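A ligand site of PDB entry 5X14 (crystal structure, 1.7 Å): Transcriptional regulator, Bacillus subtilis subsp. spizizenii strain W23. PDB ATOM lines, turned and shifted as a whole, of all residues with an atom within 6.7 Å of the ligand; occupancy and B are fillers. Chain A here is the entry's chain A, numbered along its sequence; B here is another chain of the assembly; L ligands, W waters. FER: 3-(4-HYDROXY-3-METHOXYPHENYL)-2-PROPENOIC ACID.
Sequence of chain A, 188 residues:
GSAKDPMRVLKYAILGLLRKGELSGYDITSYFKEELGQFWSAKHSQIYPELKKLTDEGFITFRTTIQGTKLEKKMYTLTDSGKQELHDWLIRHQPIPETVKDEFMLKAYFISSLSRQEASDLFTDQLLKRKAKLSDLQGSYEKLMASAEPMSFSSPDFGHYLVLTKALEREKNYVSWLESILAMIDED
Residues that only touch the ligand: Glu 35 (3.7 Å), Gln 38 (3.8 Å), Phe 39 (3.6 Å), Leu 137 (3.8 Å), Val 163 (3.9 Å), Leu 164 (3.4 Å) and Ala 167 (3.5 Å).
Hydrophobic or aromatic side chains that line the ligand: Phe 39, Leu 137, His 160, Val 163, Leu 164 and Ala 167.
11 residues have an atom within 4 Å of the ligand: Glu 35, Gln 38, Phe 39, Leu 137, Ser 140, His 160, Val 163, Leu 164, Ala 167, Arg 170 and Thr 99 of chain B.
The nearest printed residue that does not touch the ligand is Lys 133 (4.1 Å).
Water W1 lies within hydrogen-bond range of O1 of the ligand (2.5 Å), NZ of Lys 133 (2.6 Å), OE1 of Gln 38 (3.3 Å) and OG1 of Thr 99 of chain B (3.4 Å).
Water W2 bridges O2 of the ligand (3.0 Å) and O of Val 163 (3.0 Å).
OG1 of Thr 99 of chain B sits at hydrogen-bond distance from O1 of the ligand (2.6 Å).
An oxygen (O1) of the ligand lies within salt-bridge range of the guanidinium group (NH2) of Arg 170 (2.7 Å).
An oxygen (O3) of the ligand lies close to the side-chain hydroxyl of Ser 140, at 2.8 Å.
An oxygen (O4) of the ligand lies within hydrogen-bond range of a ring nitrogen (NE2) of His 160 (2.9 Å).
OG1 of Thr 99 of chain B sits at hydrogen-bond distance from NH2 of Arg 170 (3.4 Å).
The guanidinium group (NH2) of Arg 170 is in salt-bridge range of the side-chain carboxylate (OE2) of Glu 171 (3.0 Å).
The side-chain hydroxyl (OG) of Ser 140 lies within hydrogen-bond range of the backbone carbonyl oxygen (O) of Asp 136 (3.4 Å).
ND1 of His 160 lies within hydrogen-bond range of OE2 of Glu 35, 3.4 Å away.
OE2 of Glu 35 lies within hydrogen-bond range of OH of Tyr 109 of chain B.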
ATOM      1  N   GLU A  34       2.679 -10.640  20.277  1.00  0.00           N
ATOM      2  CA  GLU A  34       3.006 -10.954  18.886  1.00  0.00           C
ATOM      3  C   GLU A  34       3.330 -12.454  18.716  1.00  0.00           C
ATOM      4  O   GLU A  34       2.513 -13.301  19.108  1.00  0.00           O
ATOM      5  CB  GLU A  34       4.141 -10.029  18.392  1.00  0.00           C
ATOM      6  CG  GLU A  34       3.849  -8.528  18.561  1.00  0.00           C
ATOM      7  N   GLU A  35       4.508 -12.766  18.180  1.00  0.00           N
ATOM      8  CA  GLU A  35       4.838 -14.102  17.666  1.00  0.00           C
ATOM      9  C   GLU A  35       4.723 -15.234  18.689  1.00  0.00           C
ATOM     10  O   GLU A  35       4.167 -16.293  18.397  1.00  0.00           O
ATOM     11  CB  GLU A  35       6.227 -14.104  16.945  1.00  0.00           C
ATOM     12  CG  GLU A  35       7.394 -13.795  17.850  1.00  0.00           C
ATOM     13  CD  GLU A  35       8.711 -13.389  17.150  1.00  0.00           C
ATOM     14  OE1 GLU A  35       8.815 -12.294  16.552  1.00  0.00           O
ATOM     15  OE2 GLU A  35       9.683 -14.125  17.281  1.00  0.00           O
ATOM     16  N   LEU A  36       5.217 -14.989  19.902  1.00  0.00           N
ATOM     17  CA  LEU A  36       5.267 -16.021  20.924  1.00  0.00           C
ATOM     18  C   LEU A  36       3.854 -16.349  21.437  1.00  0.00           C
ATOM     19  O   LEU A  36       3.603 -17.498  21.781  1.00  0.00           O
ATOM     20  CB  LEU A  36       6.207 -15.576  22.050  1.00  0.00           C
ATOM     21  CG  LEU A  36       6.407 -16.423  23.301  1.00  0.00           C
ATOM     22  CD1 LEU A  36       6.999 -17.777  22.910  1.00  0.00           C
ATOM     23  CD2 LEU A  36       7.373 -15.686  24.280  1.00  0.00           C
ATOM     24  N   GLN A  38       1.250 -16.648  19.690  1.00  0.00           N
ATOM     25  CA  GLN A  38       0.519 -17.430  18.704  1.00  0.00           C
ATOM     26  C   GLN A  38       0.631 -18.933  19.000  1.00  0.00           C
ATOM     27  O   GLN A  38      -0.291 -19.657  18.696  1.00  0.00           O
ATOM     28  CB  GLN A  38       1.011 -17.102  17.285  1.00  0.00           C
ATOM     29  CG  GLN A  38       0.573 -15.731  16.824  1.00  0.00           C
ATOM     30  CD  GLN A  38      -0.907 -15.671  16.537  1.00  0.00           C
ATOM     31  OE1 GLN A  38      -1.402 -16.293  15.574  1.00  0.00           O
ATOM     32  NE2 GLN A  38      -1.622 -14.922  17.345  1.00  0.00           N
ATOM     33  N   PHE A  39       1.725 -19.382  19.583  1.00  0.00           N
ATOM     34  CA  PHE A  39       1.896 -20.823  19.944  1.00  0.00           C
ATOM     35  C   PHE A  39       2.162 -21.067  21.449  1.00  0.00           C
ATOM     36  O   PHE A  39       2.221 -22.212  21.913  1.00  0.00           O
ATOM     37  CB  PHE A  39       2.974 -21.430  19.072  1.00  0.00           C
ATOM     38  CG  PHE A  39       4.362 -20.922  19.395  1.00  0.00           C
ATOM     39  CD1 PHE A  39       4.820 -19.720  18.870  1.00  0.00           C
ATOM     40  CD2 PHE A  39       5.190 -21.639  20.242  1.00  0.00           C
ATOM     41  CE1 PHE A  39       6.088 -19.231  19.218  1.00  0.00           C
ATOM     42  CE2 PHE A  39       6.473 -21.153  20.574  1.00  0.00           C
ATOM     43  CZ  PHE A  39       6.895 -19.948  20.070  1.00  0.00           C
ATOM     44  N   LYS A 133      -6.649 -19.257   8.013  1.00  0.00           N
ATOM     45  CA  LYS A 133      -5.549 -19.281   8.999  1.00  0.00           C
ATOM     46  C   LYS A 133      -4.237 -19.545   8.284  1.00  0.00           C
ATOM     47  O   LYS A 133      -3.218 -18.933   8.582  1.00  0.00           O
ATOM     48  CB  LYS A 133      -5.784 -20.346  10.056  1.00  0.00           C
ATOM     49  CG  LYS A 133      -4.726 -20.416  11.106  1.00  0.00           C
ATOM     50  CD  LYS A 133      -5.072 -21.393  12.194  1.00  0.00           C
ATOM     51  CE  LYS A 133      -4.001 -21.352  13.304  1.00  0.00           C
ATOM     52  NZ  LYS A 133      -4.133 -20.061  14.037  1.00  0.00           N
ATOM     53  N   ASP A 136      -2.916 -16.467   6.695  1.00  0.00           N
ATOM     54  CA  ASP A 136      -2.301 -15.629   7.708  1.00  0.00           C
ATOM     55  C   ASP A 136      -0.888 -16.098   8.065  1.00  0.00           C
ATOM     56  O   ASP A 136       0.036 -15.286   8.164  1.00  0.00           O
ATOM     57  CB  ASP A 136      -3.142 -15.612   9.000  1.00  0.00           C
ATOM     58  CG  ASP A 136      -4.513 -14.990   8.818  1.00  0.00           C
ATOM     59  OD1 ASP A 136      -4.765 -14.307   7.800  1.00  0.00           O
ATOM     60  OD2 ASP A 136      -5.408 -15.234   9.703  1.00  0.00           O
ATOM     61  N   LEU A 137      -0.727 -17.412   8.249  1.00  0.00           N
ATOM     62  CA  LEU A 137       0.619 -17.972   8.547  1.00  0.00           C
ATOM     63  C   LEU A 137       1.563 -17.749   7.392  1.00  0.00           C
ATOM     64  O   LEU A 137       2.737 -17.451   7.625  1.00  0.00           O
ATOM     65  CB  LEU A 137       0.527 -19.458   8.856  1.00  0.00           C
ATOM     66  CG  LEU A 137      -0.208 -19.748  10.152  1.00  0.00           C
ATOM     67  CD1 LEU A 137      -0.513 -21.258  10.256  1.00  0.00           C
ATOM     68  CD2 LEU A 137       0.634 -19.281  11.330  1.00  0.00           C
ATOM     69  N   GLY A 139       1.545 -15.309   5.271  1.00  0.00           N
ATOM     70  CA  GLY A 139       1.954 -13.893   5.372  1.00  0.00           C
ATOM     71  C   GLY A 139       3.057 -13.638   6.391  1.00  0.00           C
ATOM     72  O   GLY A 139       4.027 -12.912   6.139  1.00  0.00           O
ATOM     73  N   SER A 140       2.942 -14.271   7.559  1.00  0.00           N
ATOM     74  CA  SER A 140       3.945 -14.125   8.611  1.00  0.00           C
ATOM     75  C   SER A 140       5.271 -14.741   8.156  1.00  0.00           C
ATOM     76  O   SER A 140       6.342 -14.222   8.450  1.00  0.00           O
ATOM     77  CB  SER A 140       3.458 -14.817   9.883  1.00  0.00           C
ATOM     78  OG  SER A 140       2.338 -14.116  10.428  1.00  0.00           O
ATOM     79  N   TYR A 141       5.151 -15.896   7.498  1.00  0.00           N
ATOM     80  CA  TYR A 141       6.321 -16.585   6.953  1.00  0.00           C
ATOM     81  C   TYR A 141       7.040 -15.695   5.909  1.00  0.00           C
ATOM     82  O   TYR A 141       8.264 -15.501   5.948  1.00  0.00           O
ATOM     83  CB  TYR A 141       5.898 -17.915   6.341  1.00  0.00           C
ATOM     84  CG  TYR A 141       6.997 -18.685   5.702  1.00  0.00           C
ATOM     85  CD1 TYR A 141       8.029 -19.254   6.460  1.00  0.00           C
ATOM     86  CD2 TYR A 141       6.995 -18.900   4.341  1.00  0.00           C
ATOM     87  CE1 TYR A 141       9.046 -19.970   5.836  1.00  0.00           C
ATOM     88  CE2 TYR A 141       8.002 -19.627   3.717  1.00  0.00           C
ATOM     89  CZ  TYR A 141       9.004 -20.160   4.457  1.00  0.00           C
ATOM     90  OH  TYR A 141       9.992 -20.872   3.781  1.00  0.00           O
ATOM     91  N   LEU A 144       8.975 -12.926   7.661  1.00  0.00           N
ATOM     92  CA  LEU A 144      10.216 -13.399   8.249  1.00  0.00           C
ATOM     93  C   LEU A 144      11.272 -13.570   7.156  1.00  0.00           C
ATOM     94  O   LEU A 144      12.427 -13.219   7.359  1.00  0.00           O
ATOM     95  CB  LEU A 144      10.019 -14.776   8.927  1.00  0.00           C
ATOM     96  CG  LEU A 144      11.242 -15.459   9.470  1.00  0.00           C
ATOM     97  CD1 LEU A 144      11.874 -14.607  10.571  1.00  0.00           C
ATOM     98  CD2 LEU A 144      10.869 -16.865   9.957  1.00  0.00           C
ATOM     99  N   HIS A 160      12.645 -18.864  15.006  1.00  0.00           N
ATOM    100  CA  HIS A 160      11.395 -18.316  14.502  1.00  0.00           C
ATOM    101  C   HIS A 160      10.928 -19.072  13.241  1.00  0.00           C
ATOM    102  O   HIS A 160       9.757 -19.408  13.094  1.00  0.00           O
ATOM    103  CB  HIS A 160      11.581 -16.828  14.187  1.00  0.00           C
ATOM    104  CG  HIS A 160      10.322 -16.068  14.033  1.00  0.00           C
ATOM    105  ND1 HIS A 160      10.315 -14.689  13.950  1.00  0.00           N
ATOM    106  CD2 HIS A 160       9.028 -16.465  13.985  1.00  0.00           C
ATOM    107  CE1 HIS A 160       9.054 -14.282  13.836  1.00  0.00           C
ATOM    108  NE2 HIS A 160       8.258 -15.332  13.870  1.00  0.00           N
ATOM    109  N   VAL A 163       9.333 -22.439  14.281  1.00  0.00           N
ATOM    110  CA  VAL A 163       7.921 -22.385  14.745  1.00  0.00           C
ATOM    111  C   VAL A 163       6.943 -22.059  13.595  1.00  0.00           C
ATOM    112  O   VAL A 163       5.860 -22.609  13.563  1.00  0.00           O
ATOM    113  CB  VAL A 163       7.669 -21.466  15.984  1.00  0.00           C
ATOM    114  CG1 VAL A 163       8.277 -22.078  17.202  1.00  0.00           C
ATOM    115  CG2 VAL A 163       8.135 -20.012  15.768  1.00  0.00           C
ATOM    116  N   LEU A 164       7.353 -21.189  12.672  1.00  0.00           N
ATOM    117  CA  LEU A 164       6.470 -20.775  11.601  1.00  0.00           C
ATOM    118  C   LEU A 164       6.304 -21.879  10.615  1.00  0.00           C
ATOM    119  O   LEU A 164       5.180 -22.159  10.177  1.00  0.00           O
ATOM    120  CB  LEU A 164       6.963 -19.514  10.952  1.00  0.00           C
ATOM    121  CG  LEU A 164       6.303 -18.249  11.444  1.00  0.00           C
ATOM    122  CD1 LEU A 164       7.058 -17.052  10.897  1.00  0.00           C
ATOM    123  CD2 LEU A 164       4.848 -18.346  10.926  1.00  0.00           C
ATOM    124  N   LYS A 166       6.643 -25.108  11.171  1.00  0.00           N
ATOM    125  CA  LYS A 166       5.843 -26.122  11.817  1.00  0.00           C
ATOM    126  C   LYS A 166       4.337 -25.802  11.721  1.00  0.00           C
ATOM    127  O   LYS A 166       3.523 -26.639  11.370  1.00  0.00           O
ATOM    128  CB  LYS A 166       6.246 -26.271  13.271  1.00  0.00           C
ATOM    129  CG  LYS A 166       5.492 -27.323  14.037  1.00  0.00           C
ATOM    130  CD  LYS A 166       5.910 -28.724  13.577  1.00  0.00           C
ATOM    131  CE  LYS A 166       5.354 -29.796  14.426  1.00  0.00           C
ATOM    132  NZ  LYS A 166       3.982 -30.151  13.980  1.00  0.00           N
ATOM    133  N   ALA A 167       3.997 -24.547  11.985  1.00  0.00           N
ATOM    134  CA  ALA A 167       2.578 -24.122  11.992  1.00  0.00           C
ATOM    135  C   ALA A 167       2.005 -24.219  10.577  1.00  0.00           C
ATOM    136  O   ALA A 167       0.871 -24.625  10.396  1.00  0.00           O
ATOM    137  CB  ALA A 167       2.447 -22.696  12.539  1.00  0.00           C
ATOM    138  N   LEU A 168       2.794 -23.820   9.589  1.00  0.00           N
ATOM    139  CA  LEU A 168       2.358 -23.875   8.190  1.00  0.00           C
ATOM    140  C   LEU A 168       2.107 -25.266   7.784  1.00  0.00           C
ATOM    141  O   LEU A 168       1.071 -25.542   7.165  1.00  0.00           O
ATOM    142  CB  LEU A 168       3.424 -23.312   7.269  1.00  0.00           C
ATOM    143  CG  LEU A 168       3.508 -21.842   7.199  1.00  0.00           C
ATOM    144  CD1 LEU A 168       4.870 -21.540   6.528  1.00  0.00           C
ATOM    145  CD2 LEU A 168       2.337 -21.277   6.337  1.00  0.00           C
ATOM    146  N   ARG A 170       1.499 -27.805   9.678  1.00  0.00           N
ATOM    147  CA  ARG A 170       0.344 -28.283  10.508  1.00  0.00           C
ATOM    148  C   ARG A 170      -1.003 -27.935   9.859  1.00  0.00           C
ATOM    149  O   ARG A 170      -1.918 -28.793   9.668  1.00  0.00           O
ATOM    150  CB  ARG A 170       0.417 -27.698  11.919  1.00  0.00           C
ATOM    151  CG  ARG A 170      -0.649 -28.213  12.902  1.00  0.00           C
ATOM    152  CD  ARG A 170      -0.525 -27.486  14.257  1.00  0.00           C
ATOM    153  NE  ARG A 170      -1.012 -26.133  14.034  1.00  0.00           N
ATOM    154  CZ  ARG A 170      -0.482 -25.019  14.487  1.00  0.00           C
ATOM    155  NH1 ARG A 170       0.559 -25.024  15.289  1.00  0.00           N
ATOM    156  NH2 ARG A 170      -1.032 -23.869  14.107  1.00  0.00           N
ATOM    157  N   GLU A 171      -1.142 -26.672   9.491  1.00  0.00           N
ATOM    158  CA  GLU A 171      -2.400 -26.202   8.931  1.00  0.00           C
ATOM    159  C   GLU A 171      -2.577 -26.707   7.524  1.00  0.00           C
ATOM    160  O   GLU A 171      -3.693 -27.068   7.131  1.00  0.00           O
ATOM    161  CB  GLU A 171      -2.530 -24.713   8.999  1.00  0.00           C
ATOM    162  CG  GLU A 171      -2.548 -24.162  10.414  1.00  0.00           C
ATOM    163  CD  GLU A 171      -3.642 -24.729  11.285  1.00  0.00           C
ATOM    164  OE1 GLU A 171      -4.774 -25.042  10.735  1.00  0.00           O
ATOM    165  OE2 GLU A 171      -3.362 -24.927  12.471  1.00  0.00           O
ATOM    166  N   GLU B  98      -7.132 -21.323  19.825  1.00  0.00           N
ATOM    167  CA  GLU B  98      -5.709 -21.054  20.030  1.00  0.00           C
ATOM    168  C   GLU B  98      -4.883 -22.324  19.908  1.00  0.00           C
ATOM    169  O   GLU B  98      -5.290 -23.433  20.273  1.00  0.00           O
ATOM    170  CB  GLU B  98      -5.494 -20.359  21.408  1.00  0.00           C
ATOM    171  N   THR B  99      -3.667 -22.163  19.384  1.00  0.00           N
ATOM    172  CA  THR B  99      -2.765 -23.276  19.178  1.00  0.00           C
ATOM    173  C   THR B  99      -2.400 -23.921  20.465  1.00  0.00           C
ATOM    174  O   THR B  99      -2.104 -23.191  21.470  1.00  0.00           O
ATOM    175  CB  THR B  99      -1.511 -22.734  18.380  1.00  0.00           C
ATOM    176  OG1 THR B  99      -1.941 -22.484  17.031  1.00  0.00           O
ATOM    177  CG2 THR B  99      -0.303 -23.725  18.346  1.00  0.00           C
ATOM    178  N   VAL B 100      -2.426 -25.244  20.491  1.00  0.00           N
ATOM    179  CA  VAL B 100      -2.140 -25.961  21.753  1.00  0.00           C
ATOM    180  C   VAL B 100      -0.664 -25.867  22.030  1.00  0.00           C
ATOM    181  O   VAL B 100       0.121 -25.987  21.083  1.00  0.00           O
ATOM    182  CB  VAL B 100      -2.489 -27.428  21.682  1.00  0.00           C
ATOM    183  CG1 VAL B 100      -2.057 -28.110  23.009  1.00  0.00           C
ATOM    184  CG2 VAL B 100      -3.976 -27.559  21.423  1.00  0.00           C
ATOM    185  N   TYR B 109      12.002 -22.939  19.289  1.00  0.00           N
ATOM    186  CA  TYR B 109      12.025 -21.473  19.213  1.00  0.00           C
ATOM    187  C   TYR B 109      13.333 -20.890  19.816  1.00  0.00           C
ATOM    188  O   TYR B 109      13.932 -19.923  19.287  1.00  0.00           O
ATOM    189  CB  TYR B 109      10.817 -20.897  19.917  1.00  0.00           C
ATOM    190  CG  TYR B 109      10.604 -19.397  19.776  1.00  0.00           C
ATOM    191  CD1 TYR B 109      10.427 -18.804  18.503  1.00  0.00           C
ATOM    192  CD2 TYR B 109      10.514 -18.593  20.877  1.00  0.00           C
ATOM    193  CE1 TYR B 109      10.204 -17.452  18.388  1.00  0.00           C
ATOM    194  CE2 TYR B 109      10.295 -17.246  20.785  1.00  0.00           C
ATOM    195  CZ  TYR B 109      10.150 -16.660  19.556  1.00  0.00           C
ATOM    196  OH  TYR B 109       9.903 -15.296  19.527  1.00  0.00           O
HETATM  197  C4  FER L   1       4.775 -16.198  13.862  1.00  0.00           C
HETATM  198  C5  FER L   1       5.462 -17.208  14.576  1.00  0.00           C
HETATM  199  C6  FER L   1       4.744 -18.365  14.961  1.00  0.00           C
HETATM  200  C3  FER L   1       3.324 -16.370  13.559  1.00  0.00           C
HETATM  201  C2  FER L   1       2.690 -17.562  13.956  1.00  0.00           C
HETATM  202  C1  FER L   1       3.399 -18.553  14.661  1.00  0.00           C
HETATM  203  C10 FER L   1       1.236 -15.595  12.498  1.00  0.00           C
HETATM  204  C7  FER L   1       2.767 -19.830  15.125  1.00  0.00           C
HETATM  205  C8  FER L   1       1.478 -20.082  14.997  1.00  0.00           C
HETATM  206  C9  FER L   1       0.878 -21.349  15.456  1.00  0.00           C
HETATM  207  O1  FER L   1      -0.359 -21.478  15.278  1.00  0.00           O
HETATM  208  O2  FER L   1       1.561 -22.305  15.918  1.00  0.00           O
HETATM  209  O4  FER L   1       5.436 -15.067  13.467  1.00  0.00           O
HETATM  210  O3  FER L   1       2.637 -15.406  12.868  1.00  0.00           O
HETATM  211  O   HOH W   1      -1.898 -19.565  15.313  1.00  0.00           O
HETATM  212  O   HOH W   2       4.199 -23.684  15.859  1.00  0.00           O
